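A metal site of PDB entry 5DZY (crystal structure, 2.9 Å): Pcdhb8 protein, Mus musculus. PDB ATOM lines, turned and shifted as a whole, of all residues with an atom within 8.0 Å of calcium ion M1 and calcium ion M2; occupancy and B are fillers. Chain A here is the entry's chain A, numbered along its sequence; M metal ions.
The side-chain carboxylate (OE2) of Glu 175 lies close to the guanidinium group (NH1) of Arg 174. OD2 of Asp 242 lies close to OD1 of Asn 208 (2.8 Å). N of Ala 243 lies within hydrogen-bond range of OD2 of Asp 206, at 3.2 Å. N of Asn 210 is in hydrogen-bond range of OD2 of Asp 242, 3.2 Å away. O of Val 205 is in hydrogen-bond range of N of Glu 116, 3.2 Å away. OD1 of Asp 240 is in hydrogen-bond range of N of Asp 242. OD1 of Asp 206 is in salt-bridge range of NE of Arg 174. ND2 of Asn 210 lies close to OD1 of Asp 209 (2.8 Å).
Residues that only touch calcium ion M1: Asn 210. Of the 19 residues printed, 7 come within 4 Å of calcium ion M1.
Residues that only touch calcium ion M2: Asn 210.
Calcium ion M1 is bound by OE2 of Glu 175 (2.3 Å), O of Ile 207 (2.4 Å), OD1 of Asp 209 (2.4 Å), OE1 of Glu 116 (2.4 Å) and OD1 of Asp 242 (2.5 Å). Slightly farther from calcium ion M1 lies the side-chain carboxylate (OE1) of Glu 175 (2.9 Å). Slightly farther from calcium ion M1 lies OD1 of Asp 206 (3.0 Å).
Calcium ion M2 is bound by OE2 of Glu 116 (2.2 Å), OD2 of Asp 209 (2.3 Å), OD1 of Asp 173 (2.5 Å) and OE1 of Glu 175 (2.5 Å). Slightly farther from calcium ion M2 lies the side-chain carboxylate (OD1) of Asp 209 (3.1 Å).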
ATOM      1  N   GLU A 116      18.512   6.270 -19.867  1.00  0.00           N
ATOM      2  CA  GLU A 116      19.236   5.033 -20.160  1.00  0.00           C
ATOM      3  C   GLU A 116      20.695   5.275 -20.540  1.00  0.00           C
ATOM      4  O   GLU A 116      21.571   4.485 -20.187  1.00  0.00           O
ATOM      5  CB  GLU A 116      18.530   4.267 -21.274  1.00  0.00           C
ATOM      6  CG  GLU A 116      19.169   2.946 -21.671  1.00  0.00           C
ATOM      7  CD  GLU A 116      18.459   2.291 -22.840  1.00  0.00           C
ATOM      8  OE1 GLU A 116      17.496   2.898 -23.365  1.00  0.00           O
ATOM      9  OE2 GLU A 116      18.854   1.182 -23.245  1.00  0.00           O
ATOM     10  N   ILE A 117      20.961   6.361 -21.253  1.00  0.00           N
ATOM     11  CA  ILE A 117      22.316   6.641 -21.742  1.00  0.00           C
ATOM     12  C   ILE A 117      23.175   7.403 -20.732  1.00  0.00           C
ATOM     13  O   ILE A 117      24.166   8.026 -21.111  1.00  0.00           O
ATOM     14  CB  ILE A 117      22.280   7.454 -23.050  1.00  0.00           C
ATOM     15  CG1 ILE A 117      21.434   8.721 -22.867  1.00  0.00           C
ATOM     16  CG2 ILE A 117      21.760   6.610 -24.196  1.00  0.00           C
ATOM     17  CD1 ILE A 117      21.357   9.581 -24.112  1.00  0.00           C
ATOM     18  N   LEU A 172      22.909   1.813 -17.411  1.00  0.00           N
ATOM     19  CA  LEU A 172      21.591   1.183 -17.318  1.00  0.00           C
ATOM     20  C   LEU A 172      21.090   0.722 -18.674  1.00  0.00           C
ATOM     21  O   LEU A 172      21.684   1.011 -19.714  1.00  0.00           O
ATOM     22  CB  LEU A 172      20.584   2.150 -16.691  1.00  0.00           C
ATOM     23  CG  LEU A 172      20.898   2.669 -15.280  1.00  0.00           C
ATOM     24  CD1 LEU A 172      19.859   3.681 -14.851  1.00  0.00           C
ATOM     25  CD2 LEU A 172      20.968   1.515 -14.301  1.00  0.00           C
ATOM     26  N   ASP A 173      19.960   0.007 -18.664  1.00  0.00           N
ATOM     27  CA  ASP A 173      19.335  -0.467 -19.892  1.00  0.00           C
ATOM     28  C   ASP A 173      17.878  -0.846 -19.626  1.00  0.00           C
ATOM     29  O   ASP A 173      17.604  -1.813 -18.909  1.00  0.00           O
ATOM     30  CB  ASP A 173      20.097  -1.673 -20.460  1.00  0.00           C
ATOM     31  CG  ASP A 173      19.600  -2.070 -21.844  1.00  0.00           C
ATOM     32  OD1 ASP A 173      20.130  -1.527 -22.839  1.00  0.00           O
ATOM     33  OD2 ASP A 173      18.692  -2.923 -21.926  1.00  0.00           O
ATOM     34  N   ARG A 174      16.954  -0.074 -20.191  1.00  0.00           N
ATOM     35  CA  ARG A 174      15.531  -0.303 -19.973  1.00  0.00           C
ATOM     36  C   ARG A 174      15.072  -1.608 -20.623  1.00  0.00           C
ATOM     37  O   ARG A 174      14.117  -2.238 -20.172  1.00  0.00           O
ATOM     38  CB  ARG A 174      14.709   0.865 -20.524  1.00  0.00           C
ATOM     39  CG  ARG A 174      13.241   0.819 -20.130  1.00  0.00           C
ATOM     40  CD  ARG A 174      12.399   1.748 -20.984  1.00  0.00           C
ATOM     41  NE  ARG A 174      12.442   1.361 -22.385  1.00  0.00           N
ATOM     42  CZ  ARG A 174      11.637   0.459 -22.941  1.00  0.00           C
ATOM     43  NH1 ARG A 174      11.743   0.182 -24.233  1.00  0.00           N
ATOM     44  NH2 ARG A 174      10.735  -0.161 -22.206  1.00  0.00           N
ATOM     45  N   GLU A 175      15.765  -2.006 -21.692  1.00  0.00           N
ATOM     46  CA  GLU A 175      15.431  -3.223 -22.408  1.00  0.00           C
ATOM     47  C   GLU A 175      15.796  -4.460 -21.586  1.00  0.00           C
ATOM     48  O   GLU A 175      15.306  -5.555 -21.841  1.00  0.00           O
ATOM     49  CB  GLU A 175      16.132  -3.265 -23.764  1.00  0.00           C
ATOM     50  CG  GLU A 175      15.552  -2.293 -24.793  1.00  0.00           C
ATOM     51  CD  GLU A 175      15.834  -0.837 -24.463  1.00  0.00           C
ATOM     52  OE1 GLU A 175      16.885  -0.559 -23.856  1.00  0.00           O
ATOM     53  OE2 GLU A 175      14.992   0.026 -24.793  1.00  0.00           O
ATOM     54  N   GLU A 176      16.670  -4.267 -20.593  1.00  0.00           N
ATOM     55  CA  GLU A 176      17.054  -5.342 -19.691  1.00  0.00           C
ATOM     56  C   GLU A 176      16.313  -5.233 -18.365  1.00  0.00           C
ATOM     57  O   GLU A 176      15.572  -6.133 -17.980  1.00  0.00           O
ATOM     58  CB  GLU A 176      18.563  -5.328 -19.463  1.00  0.00           C
ATOM     59  N   VAL A 204      14.049   4.033 -14.946  1.00  0.00           N
ATOM     60  CA  VAL A 204      14.881   4.194 -16.130  1.00  0.00           C
ATOM     61  C   VAL A 204      14.085   4.754 -17.308  1.00  0.00           C
ATOM     62  O   VAL A 204      13.216   4.077 -17.865  1.00  0.00           O
ATOM     63  CB  VAL A 204      15.535   2.863 -16.555  1.00  0.00           C
ATOM     64  CG1 VAL A 204      16.386   3.057 -17.794  1.00  0.00           C
ATOM     65  CG2 VAL A 204      16.374   2.305 -15.417  1.00  0.00           C
ATOM     66  N   VAL A 205      14.401   5.986 -17.694  1.00  0.00           N
ATOM     67  CA  VAL A 205      13.732   6.631 -18.817  1.00  0.00           C
ATOM     68  C   VAL A 205      14.203   6.033 -20.142  1.00  0.00           C
ATOM     69  O   VAL A 205      15.402   5.849 -20.347  1.00  0.00           O
ATOM     70  CB  VAL A 205      13.991   8.158 -18.830  1.00  0.00           C
ATOM     71  CG1 VAL A 205      13.276   8.807 -20.005  1.00  0.00           C
ATOM     72  CG2 VAL A 205      13.544   8.775 -17.516  1.00  0.00           C
ATOM     73  N   ASP A 206      13.259   5.727 -21.023  1.00  0.00           N
ATOM     74  CA  ASP A 206      13.589   5.107 -22.311  1.00  0.00           C
ATOM     75  C   ASP A 206      14.386   6.041 -23.223  1.00  0.00           C
ATOM     76  O   ASP A 206      14.037   7.206 -23.388  1.00  0.00           O
ATOM     77  CB  ASP A 206      12.310   4.670 -23.029  1.00  0.00           C
ATOM     78  CG  ASP A 206      12.587   4.020 -24.366  1.00  0.00           C
ATOM     79  OD1 ASP A 206      13.639   3.364 -24.507  1.00  0.00           O
ATOM     80  OD2 ASP A 206      11.745   4.158 -25.289  1.00  0.00           O
ATOM     81  N   ILE A 207      15.442   5.494 -23.822  1.00  0.00           N
ATOM     82  CA  ILE A 207      16.207   6.224 -24.830  1.00  0.00           C
ATOM     83  C   ILE A 207      16.260   5.409 -26.115  1.00  0.00           C
ATOM     84  O   ILE A 207      16.484   4.203 -26.081  1.00  0.00           O
ATOM     85  CB  ILE A 207      17.647   6.532 -24.340  1.00  0.00           C
ATOM     86  CG1 ILE A 207      17.619   7.338 -23.042  1.00  0.00           C
ATOM     87  CG2 ILE A 207      18.416   7.299 -25.404  1.00  0.00           C
ATOM     88  CD1 ILE A 207      16.978   8.700 -23.186  1.00  0.00           C
ATOM     89  N   ASN A 208      16.028   6.075 -27.251  1.00  0.00           N
ATOM     90  CA  ASN A 208      16.041   5.405 -28.547  1.00  0.00           C
ATOM     91  C   ASN A 208      17.452   4.999 -28.936  1.00  0.00           C
ATOM     92  O   ASN A 208      18.135   5.722 -29.674  1.00  0.00           O
ATOM     93  CB  ASN A 208      15.419   6.297 -29.618  1.00  0.00           C
ATOM     94  CG  ASN A 208      15.299   5.605 -30.977  1.00  0.00           C
ATOM     95  OD1 ASN A 208      15.472   4.388 -31.086  1.00  0.00           O
ATOM     96  ND2 ASN A 208      15.001   6.378 -32.009  1.00  0.00           N
ATOM     97  N   ASP A 209      17.902   3.861 -28.426  1.00  0.00           N
ATOM     98  CA  ASP A 209      19.230   3.344 -28.734  1.00  0.00           C
ATOM     99  C   ASP A 209      19.122   2.056 -29.552  1.00  0.00           C
ATOM    100  O   ASP A 209      20.118   1.425 -29.880  1.00  0.00           O
ATOM    101  CB  ASP A 209      20.030   3.110 -27.446  1.00  0.00           C
ATOM    102  CG  ASP A 209      19.319   2.177 -26.480  1.00  0.00           C
ATOM    103  OD1 ASP A 209      18.108   1.927 -26.654  1.00  0.00           O
ATOM    104  OD2 ASP A 209      19.983   1.692 -25.530  1.00  0.00           O
ATOM    105  N   ASN A 210      17.886   1.683 -29.882  1.00  0.00           N
ATOM    106  CA  ASN A 210      17.631   0.507 -30.701  1.00  0.00           C
ATOM    107  C   ASN A 210      17.026   0.870 -32.057  1.00  0.00           C
ATOM    108  O   ASN A 210      16.110   1.683 -32.142  1.00  0.00           O
ATOM    109  CB  ASN A 210      16.710  -0.473 -29.971  1.00  0.00           C
ATOM    110  CG  ASN A 210      17.401  -1.170 -28.821  1.00  0.00           C
ATOM    111  OD1 ASN A 210      18.032  -2.213 -29.011  1.00  0.00           O
ATOM    112  ND2 ASN A 210      17.289  -0.602 -27.627  1.00  0.00           N
ATOM    113  N   ASP A 240      10.320  -2.622 -33.100  1.00  0.00           N
ATOM    114  CA  ASP A 240      11.320  -1.843 -32.378  1.00  0.00           C
ATOM    115  C   ASP A 240      11.404  -2.307 -30.932  1.00  0.00           C
ATOM    116  O   ASP A 240      10.391  -2.594 -30.295  1.00  0.00           O
ATOM    117  CB  ASP A 240      10.974  -0.353 -32.444  1.00  0.00           C
ATOM    118  CG  ASP A 240      12.152   0.538 -32.072  1.00  0.00           C
ATOM    119  OD1 ASP A 240      13.125   0.034 -31.479  1.00  0.00           O
ATOM    120  OD2 ASP A 240      12.085   1.752 -32.362  1.00  0.00           O
ATOM    121  N   LEU A 241      12.628  -2.383 -30.403  1.00  0.00           N
ATOM    122  CA  LEU A 241      12.846  -2.835 -29.043  1.00  0.00           C
ATOM    123  C   LEU A 241      12.521  -1.748 -28.027  1.00  0.00           C
ATOM    124  O   LEU A 241      12.243  -2.036 -26.862  1.00  0.00           O
ATOM    125  CB  LEU A 241      14.282  -3.310 -28.857  1.00  0.00           C
ATOM    126  CG  LEU A 241      14.683  -4.544 -29.679  1.00  0.00           C
ATOM    127  CD1 LEU A 241      16.121  -4.947 -29.381  1.00  0.00           C
ATOM    128  CD2 LEU A 241      13.732  -5.694 -29.413  1.00  0.00           C
ATOM    129  N   ASP A 242      12.536  -0.499 -28.470  1.00  0.00           N
ATOM    130  CA  ASP A 242      12.202   0.629 -27.600  1.00  0.00           C
ATOM    131  C   ASP A 242      10.690   0.759 -27.443  1.00  0.00           C
ATOM    132  O   ASP A 242       9.926   0.039 -28.081  1.00  0.00           O
ATOM    133  CB  ASP A 242      12.791   1.932 -28.155  1.00  0.00           C
ATOM    134  CG  ASP A 242      14.311   1.940 -28.138  1.00  0.00           C
ATOM    135  OD1 ASP A 242      14.888   1.301 -27.233  1.00  0.00           O
ATOM    136  OD2 ASP A 242      14.917   2.587 -29.022  1.00  0.00           O
ATOM    137  N   ALA A 243      10.266   1.691 -26.593  1.00  0.00           N
ATOM    138  CA  ALA A 243       8.851   1.899 -26.340  1.00  0.00           C
ATOM    139  C   ALA A 243       8.444   3.351 -26.555  1.00  0.00           C
ATOM    140  O   ALA A 243       9.293   4.236 -26.611  1.00  0.00           O
ATOM    141  CB  ALA A 243       8.498   1.463 -24.917  1.00  0.00           C
ATOM    142  N   HIS A 246       9.683   6.536 -29.281  1.00  0.00           N
ATOM    143  CA  HIS A 246      10.995   6.031 -29.682  1.00  0.00           C
ATOM    144  C   HIS A 246      10.882   4.656 -30.327  1.00  0.00           C
ATOM    145  O   HIS A 246      11.847   4.143 -30.884  1.00  0.00           O
ATOM    146  CB  HIS A 246      11.928   5.964 -28.470  1.00  0.00           C
ATOM    147  CG  HIS A 246      12.121   7.280 -27.783  1.00  0.00           C
ATOM    148  ND1 HIS A 246      13.265   8.035 -27.940  1.00  0.00           N
ATOM    149  CD2 HIS A 246      11.331   7.976 -26.940  1.00  0.00           C
ATOM    150  CE1 HIS A 246      13.167   9.143 -27.219  1.00  0.00           C
ATOM    151  NE2 HIS A 246      11.994   9.127 -26.593  1.00  0.00           N
HETATM  152 CA    CA M   1      16.153   1.952 -25.181  1.00  0.00          CA
HETATM  153 CA    CA M   2      19.185  -0.311 -24.794  1.00  0.00          CA
HETATM  154 CA    CA M   3      13.854   2.841 -31.858  1.00  0.00          CA
